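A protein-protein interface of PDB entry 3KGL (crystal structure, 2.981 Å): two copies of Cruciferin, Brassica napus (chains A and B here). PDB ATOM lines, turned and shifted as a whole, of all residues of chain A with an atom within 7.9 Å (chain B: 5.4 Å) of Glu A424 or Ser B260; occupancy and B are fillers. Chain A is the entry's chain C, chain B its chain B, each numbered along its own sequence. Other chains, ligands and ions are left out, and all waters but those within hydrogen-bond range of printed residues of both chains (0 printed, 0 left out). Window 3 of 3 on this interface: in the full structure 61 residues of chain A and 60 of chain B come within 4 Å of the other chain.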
ATOM      1  N   LEU A 421     -11.330 -26.285   6.004  1.00  0.00           N
ATOM      2  CA  LEU A 421      -9.894 -26.399   6.232  1.00  0.00           C
ATOM      3  C   LEU A 421      -9.568 -27.109   7.563  1.00  0.00           C
ATOM      4  O   LEU A 421     -10.088 -26.751   8.620  1.00  0.00           O
ATOM      5  CB  LEU A 421      -9.255 -25.007   6.235  1.00  0.00           C
ATOM      6  CG  LEU A 421      -8.465 -24.461   5.044  1.00  0.00           C
ATOM      7  CD1 LEU A 421      -8.976 -24.974   3.713  1.00  0.00           C
ATOM      8  CD2 LEU A 421      -8.499 -22.947   5.092  1.00  0.00           C
ATOM      9  N   PRO A 422      -8.711 -28.134   7.512  1.00  0.00           N
ATOM     10  CA  PRO A 422      -8.078 -28.654   8.714  1.00  0.00           C
ATOM     11  C   PRO A 422      -7.454 -27.539   9.533  1.00  0.00           C
ATOM     12  O   PRO A 422      -6.733 -26.726   8.975  1.00  0.00           O
ATOM     13  CB  PRO A 422      -6.976 -29.535   8.142  1.00  0.00           C
ATOM     14  CG  PRO A 422      -7.550 -30.055   6.907  1.00  0.00           C
ATOM     15  CD  PRO A 422      -8.396 -28.957   6.337  1.00  0.00           C
ATOM     16  N   LEU A 423      -7.704 -27.517  10.835  1.00  0.00           N
ATOM     17  CA  LEU A 423      -7.189 -26.468  11.708  1.00  0.00           C
ATOM     18  C   LEU A 423      -5.681 -26.236  11.630  1.00  0.00           C
ATOM     19  O   LEU A 423      -5.214 -25.098  11.673  1.00  0.00           O
ATOM     20  CB  LEU A 423      -7.594 -26.728  13.157  1.00  0.00           C
ATOM     21  CG  LEU A 423      -8.803 -25.906  13.594  1.00  0.00           C
ATOM     22  CD1 LEU A 423      -8.926 -25.929  15.104  1.00  0.00           C
ATOM     23  CD2 LEU A 423      -8.679 -24.470  13.083  1.00  0.00           C
ATOM     24  N   GLU A 424      -4.905 -27.302  11.530  1.00  0.00           N
ATOM     25  CA  GLU A 424      -3.462 -27.127  11.466  1.00  0.00           C
ATOM     26  C   GLU A 424      -3.040 -26.358  10.202  1.00  0.00           C
ATOM     27  O   GLU A 424      -1.955 -25.769  10.157  1.00  0.00           O
ATOM     28  CB  GLU A 424      -2.734 -28.469  11.588  1.00  0.00           C
ATOM     29  CG  GLU A 424      -2.944 -29.172  12.921  1.00  0.00           C
ATOM     30  CD  GLU A 424      -4.215 -30.020  12.962  1.00  0.00           C
ATOM     31  OE1 GLU A 424      -5.226 -29.672  12.296  1.00  0.00           O
ATOM     32  OE2 GLU A 424      -4.202 -31.043  13.679  1.00  0.00           O
ATOM     33  N   VAL A 425      -3.903 -26.359   9.185  1.00  0.00           N
ATOM     34  CA  VAL A 425      -3.689 -25.506   8.011  1.00  0.00           C
ATOM     35  C   VAL A 425      -3.980 -24.037   8.341  1.00  0.00           C
ATOM     36  O   VAL A 425      -3.174 -23.152   8.023  1.00  0.00           O
ATOM     37  CB  VAL A 425      -4.530 -25.937   6.787  1.00  0.00           C
ATOM     38  CG1 VAL A 425      -4.598 -24.799   5.781  1.00  0.00           C
ATOM     39  CG2 VAL A 425      -3.943 -27.183   6.133  1.00  0.00           C
ATOM     40  N   ILE A 426      -5.127 -23.781   8.972  1.00  0.00           N
ATOM     41  CA  ILE A 426      -5.453 -22.435   9.428  1.00  0.00           C
ATOM     42  C   ILE A 426      -4.369 -21.898  10.371  1.00  0.00           C
ATOM     43  O   ILE A 426      -3.877 -20.795  10.185  1.00  0.00           O
ATOM     44  CB  ILE A 426      -6.845 -22.375  10.100  1.00  0.00           C
ATOM     45  CG1 ILE A 426      -7.953 -22.684   9.084  1.00  0.00           C
ATOM     46  CG2 ILE A 426      -7.072 -21.030  10.824  1.00  0.00           C
ATOM     47  CD1 ILE A 426      -9.391 -22.528   9.659  1.00  0.00           C
ATOM     48  N   SER A 427      -3.968 -22.687  11.361  1.00  0.00           N
ATOM     49  CA  SER A 427      -3.045 -22.203  12.387  1.00  0.00           C
ATOM     50  C   SER A 427      -1.681 -21.867  11.821  1.00  0.00           C
ATOM     51  O   SER A 427      -1.142 -20.794  12.074  1.00  0.00           O
ATOM     52  CB  SER A 427      -2.871 -23.249  13.471  1.00  0.00           C
ATOM     53  OG  SER A 427      -2.555 -24.485  12.870  1.00  0.00           O
ATOM     54  N   ASN A 428      -1.113 -22.801  11.070  1.00  0.00           N
ATOM     55  CA  ASN A 428       0.183 -22.587  10.453  1.00  0.00           C
ATOM     56  C   ASN A 428       0.121 -21.558   9.341  1.00  0.00           C
ATOM     57  O   ASN A 428       1.031 -20.739   9.192  1.00  0.00           O
ATOM     58  CB  ASN A 428       0.711 -23.900   9.904  1.00  0.00           C
ATOM     59  CG  ASN A 428       1.412 -24.717  10.948  1.00  0.00           C
ATOM     60  OD1 ASN A 428       2.469 -24.323  11.458  1.00  0.00           O
ATOM     61  ND2 ASN A 428       0.839 -25.868  11.275  1.00  0.00           N
ATOM     62  N   GLY A 429      -0.962 -21.616   8.563  1.00  0.00           N
ATOM     63  CA  GLY A 429      -1.209 -20.688   7.473  1.00  0.00           C
ATOM     64  C   GLY A 429      -1.086 -19.232   7.883  1.00  0.00           C
ATOM     65  O   GLY A 429      -0.373 -18.469   7.241  1.00  0.00           O
ATOM     66  N   TYR A 430      -1.771 -18.835   8.956  1.00  0.00           N
ATOM     67  CA  TYR A 430      -1.793 -17.427   9.357  1.00  0.00           C
ATOM     68  C   TYR A 430      -0.865 -17.140  10.523  1.00  0.00           C
ATOM     69  O   TYR A 430      -0.694 -15.986  10.940  1.00  0.00           O
ATOM     70  CB  TYR A 430      -3.212 -16.992   9.692  1.00  0.00           C
ATOM     71  CG  TYR A 430      -4.169 -17.167   8.539  1.00  0.00           C
ATOM     72  CD1 TYR A 430      -4.272 -16.211   7.539  1.00  0.00           C
ATOM     73  CD2 TYR A 430      -4.962 -18.295   8.448  1.00  0.00           C
ATOM     74  CE1 TYR A 430      -5.145 -16.383   6.487  1.00  0.00           C
ATOM     75  CE2 TYR A 430      -5.832 -18.476   7.402  1.00  0.00           C
ATOM     76  CZ  TYR A 430      -5.923 -17.524   6.423  1.00  0.00           C
ATOM     77  OH  TYR A 430      -6.810 -17.726   5.385  1.00  0.00           O
ATOM     78  N   GLN A 431      -0.248 -18.204  11.022  1.00  0.00           N
ATOM     79  CA  GLN A 431       0.585 -18.130  12.209  1.00  0.00           C
ATOM     80  C   GLN A 431      -0.162 -17.480  13.352  1.00  0.00           C
ATOM     81  O   GLN A 431       0.105 -16.338  13.735  1.00  0.00           O
ATOM     82  CB  GLN A 431       1.901 -17.442  11.908  1.00  0.00           C
ATOM     83  CG  GLN A 431       2.813 -18.386  11.170  1.00  0.00           C
ATOM     84  CD  GLN A 431       4.101 -17.751  10.746  1.00  0.00           C
ATOM     85  OE1 GLN A 431       4.183 -16.532  10.594  1.00  0.00           O
ATOM     86  NE2 GLN A 431       5.125 -18.579  10.541  1.00  0.00           N
ATOM     87  N   ILE A 432      -1.129 -18.243  13.851  1.00  0.00           N
ATOM     88  CA  ILE A 432      -1.927 -17.901  15.007  1.00  0.00           C
ATOM     89  C   ILE A 432      -2.047 -19.150  15.899  1.00  0.00           C
ATOM     90  O   ILE A 432      -1.644 -20.260  15.514  1.00  0.00           O
ATOM     91  CB  ILE A 432      -3.338 -17.397  14.600  1.00  0.00           C
ATOM     92  CG1 ILE A 432      -4.013 -18.389  13.667  1.00  0.00           C
ATOM     93  CG2 ILE A 432      -3.271 -16.040  13.918  1.00  0.00           C
ATOM     94  CD1 ILE A 432      -5.436 -18.039  13.333  1.00  0.00           C
ATOM     95  N   LEU A 434      -3.960 -22.151  18.282  1.00  0.00           N
ATOM     96  CA  LEU A 434      -5.020 -23.111  17.985  1.00  0.00           C
ATOM     97  C   LEU A 434      -6.341 -22.583  18.522  1.00  0.00           C
ATOM     98  O   LEU A 434      -7.394 -22.851  17.948  1.00  0.00           O
ATOM     99  CB  LEU A 434      -4.722 -24.464  18.624  1.00  0.00           C
ATOM    100  CG  LEU A 434      -3.857 -25.458  17.852  1.00  0.00           C
ATOM    101  CD1 LEU A 434      -3.311 -24.845  16.573  1.00  0.00           C
ATOM    102  CD2 LEU A 434      -2.736 -25.974  18.754  1.00  0.00           C
ATOM    103  N   ALA A 437      -7.290 -20.295  15.997  1.00  0.00           N
ATOM    104  CA  ALA A 437      -7.704 -21.026  14.800  1.00  0.00           C
ATOM    105  C   ALA A 437      -9.127 -21.597  14.914  1.00  0.00           C
ATOM    106  O   ALA A 437      -9.876 -21.617  13.937  1.00  0.00           O
ATOM    107  CB  ALA A 437      -6.695 -22.123  14.457  1.00  0.00           C
ATOM    108  N   LYS A 441     -12.480 -20.305  12.542  1.00  0.00           N
ATOM    109  CA  LYS A 441     -13.137 -21.379  11.808  1.00  0.00           C
ATOM    110  C   LYS A 441     -14.606 -21.536  12.205  1.00  0.00           C
ATOM    111  O   LYS A 441     -15.442 -21.942  11.394  1.00  0.00           O
ATOM    112  CB  LYS A 441     -12.387 -22.691  12.074  1.00  0.00           C
ATOM    113  CG  LYS A 441     -12.905 -23.909  11.322  1.00  0.00           C
ATOM    114  CD  LYS A 441     -11.760 -24.868  11.025  1.00  0.00           C
ATOM    115  CE  LYS A 441     -12.270 -26.179  10.479  1.00  0.00           C
ATOM    116  NZ  LYS A 441     -12.420 -27.212  11.553  1.00  0.00           N
ATOM    117  N   LEU B  55       3.731 -27.092   3.471  1.00  0.00           N
ATOM    118  CA  LEU B  55       2.333 -26.931   3.094  1.00  0.00           C
ATOM    119  C   LEU B  55       2.166 -25.859   1.986  1.00  0.00           C
ATOM    120  O   LEU B  55       2.596 -24.705   2.149  1.00  0.00           O
ATOM    121  CB  LEU B  55       1.492 -26.589   4.329  1.00  0.00           C
ATOM    122  CG  LEU B  55      -0.014 -26.343   4.174  1.00  0.00           C
ATOM    123  CD1 LEU B  55      -0.779 -27.621   3.806  1.00  0.00           C
ATOM    124  CD2 LEU B  55      -0.576 -25.738   5.442  1.00  0.00           C
ATOM    125  N   ASP B 141     -11.665 -32.279  15.111  1.00  0.00           N
ATOM    126  CA  ASP B 141     -11.684 -31.363  13.977  1.00  0.00           C
ATOM    127  C   ASP B 141     -12.583 -31.932  12.875  1.00  0.00           C
ATOM    128  O   ASP B 141     -12.475 -33.114  12.529  1.00  0.00           O
ATOM    129  CB  ASP B 141     -10.255 -31.147  13.467  1.00  0.00           C
ATOM    130  CG  ASP B 141     -10.084 -29.846  12.680  1.00  0.00           C
ATOM    131  OD1 ASP B 141     -10.824 -28.859  12.929  1.00  0.00           O
ATOM    132  OD2 ASP B 141      -9.176 -29.820  11.819  1.00  0.00           O
ATOM    133  N   VAL B 255       5.508 -26.453   8.350  1.00  0.00           N
ATOM    134  CA  VAL B 255       4.564 -26.707   9.430  1.00  0.00           C
ATOM    135  C   VAL B 255       5.293 -26.930  10.743  1.00  0.00           C
ATOM    136  O   VAL B 255       6.154 -27.804  10.841  1.00  0.00           O
ATOM    137  CB  VAL B 255       3.685 -27.930   9.143  1.00  0.00           C
ATOM    138  CG1 VAL B 255       2.574 -28.018  10.165  1.00  0.00           C
ATOM    139  CG2 VAL B 255       3.113 -27.855   7.746  1.00  0.00           C
ATOM    140  N   PRO B 258       3.260 -31.040  14.352  1.00  0.00           N
ATOM    141  CA  PRO B 258       2.763 -32.111  13.498  1.00  0.00           C
ATOM    142  C   PRO B 258       1.625 -31.633  12.628  1.00  0.00           C
ATOM    143  O   PRO B 258       1.337 -30.434  12.530  1.00  0.00           O
ATOM    144  CB  PRO B 258       2.184 -33.070  14.518  1.00  0.00           C
ATOM    145  CG  PRO B 258       1.467 -32.108  15.466  1.00  0.00           C
ATOM    146  CD  PRO B 258       2.358 -30.844  15.503  1.00  0.00           C
ATOM    147  N   PHE B 259       0.953 -32.599  12.024  1.00  0.00           N
ATOM    148  CA  PHE B 259      -0.125 -32.302  11.114  1.00  0.00           C
ATOM    149  C   PHE B 259      -1.125 -33.435  11.181  1.00  0.00           C
ATOM    150  O   PHE B 259      -1.277 -34.205  10.230  1.00  0.00           O
ATOM    151  CB  PHE B 259       0.424 -32.150   9.700  1.00  0.00           C
ATOM    152  CG  PHE B 259      -0.403 -31.267   8.829  1.00  0.00           C
ATOM    153  CD1 PHE B 259      -0.701 -29.975   9.221  1.00  0.00           C
ATOM    154  CD2 PHE B 259      -0.886 -31.723   7.623  1.00  0.00           C
ATOM    155  CE1 PHE B 259      -1.466 -29.159   8.428  1.00  0.00           C
ATOM    156  CE2 PHE B 259      -1.650 -30.908   6.820  1.00  0.00           C
ATOM    157  CZ  PHE B 259      -1.940 -29.623   7.221  1.00  0.00           C
ATOM    158  N   SER B 260      -1.787 -33.536  12.327  1.00  0.00           N
ATOM    159  CA  SER B 260      -2.791 -34.565  12.571  1.00  0.00           C
ATOM    160  C   SER B 260      -4.074 -34.274  11.795  1.00  0.00           C
ATOM    161  O   SER B 260      -5.178 -34.320  12.343  1.00  0.00           O
ATOM    162  CB  SER B 260      -3.077 -34.668  14.070  1.00  0.00           C
ATOM    163  OG  SER B 260      -2.926 -33.407  14.705  1.00  0.00           O
ATOM    164  N   VAL B 261      -3.907 -33.976  10.510  1.00  0.00           N
ATOM    165  CA  VAL B 261      -5.009 -33.612   9.628  1.00  0.00           C
ATOM    166  C   VAL B 261      -5.964 -34.776   9.390  1.00  0.00           C
ATOM    167  O   VAL B 261      -7.141 -34.715   9.760  1.00  0.00           O
ATOM    168  CB  VAL B 261      -4.470 -33.081   8.287  1.00  0.00           C
ATOM    169  CG1 VAL B 261      -5.468 -33.319   7.168  1.00  0.00           C
ATOM    170  CG2 VAL B 261      -4.123 -31.606   8.419  1.00  0.00           C
ATOM    171  N   ILE B 262      -5.450 -35.834   8.773  1.00  0.00           N
ATOM    172  CA  ILE B 262      -6.212 -37.060   8.603  1.00  0.00           C
ATOM    173  C   ILE B 262      -5.348 -38.191   9.130  1.00  0.00           C
ATOM    174  O   ILE B 262      -4.123 -38.159   8.999  1.00  0.00           O
ATOM    175  CB  ILE B 262      -6.579 -37.314   7.120  1.00  0.00           C
ATOM    176  CG1 ILE B 262      -8.098 -37.455   6.944  1.00  0.00           C
ATOM    177  CG2 ILE B 262      -5.816 -38.506   6.560  1.00  0.00           C
ATOM    178  CD1 ILE B 262      -8.729 -38.555   7.772  1.00  0.00           C
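Printed residues of chain B within 4 Å of Glu A424: Asp B141 (3.98 Å), Phe B259 (3.5 Å) and Ser B260 (2.9 Å).
Of chain A, only Glu A424 (2.9 Å) comes within 4 Å of Ser B260.
Printed residues of chain A within 4 Å of Val B261: Pro A422.
Printed residues of chain B within 4 Å of Pro A422: Asp B141 and Val B261.
Of the printed residues of chain A, Leu B55 touches Val A425 (3.7 Å).
Of the printed residues of chain B, Lys A441 touches Asp B141 (2.7 Å).
Of the printed residues of chain A, Asp B141 touches Pro A422 (3.5 Å), Leu A423 (2.9 Å), Glu A424 (3.98 Å) and Lys A441 (2.7 Å).
The nearest printed residue of chain B that does not touch Glu A424 is Val B261 (4.3 Å).
The nearest printed residue of chain A that does not touch Val B255 is Glu A424 (5.1 Å).
Of the 8 printed residues of chain B, 6 touch a printed residue of chain A.
Hydrophobic or aromatic side chains of chain B that line the printed part of chain A: Leu B55, Val B255, Phe B259 and Val B261.
No position is printed for both chains.
The backbone NH (N) of Leu A423 sits at hydrogen-bond distance from the side-chain carboxylate (OD2) of Asp B141 (2.9 Å).
NZ of Lys A441 is in salt-bridge range of OD1 of Asp B141, 2.7 Å away.
OG of Ser B260 sits at hydrogen-bond distance from OE2 of Glu A424, at 2.9 Å.
The side-chain hydroxyl (OG) of Ser A427 sits at hydrogen-bond distance from the backbone carbonyl oxygen (O) of Leu A423 (3.0 Å).
O of Glu A424 is in hydrogen-bond range of OG of Ser A427 (3.1 Å).
O of Glu A424 is in hydrogen-bond range of ND2 of Asn A428, 3.0 Å away.
Among the printed residues, pairs that only touch across the chains: Pro A422 with Asp B141 (3.5 Å), Pro A422 with Val B261 (3.5 Å), Glu A424 with Asp B141 (3.98 Å), Glu A424 with Phe B259 (3.5 Å), Val A425 with Leu B55 (3.7 Å), Val A425 with Phe B259 (3.3 Å) and Asn A428 with Val B255 (3.0 Å).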
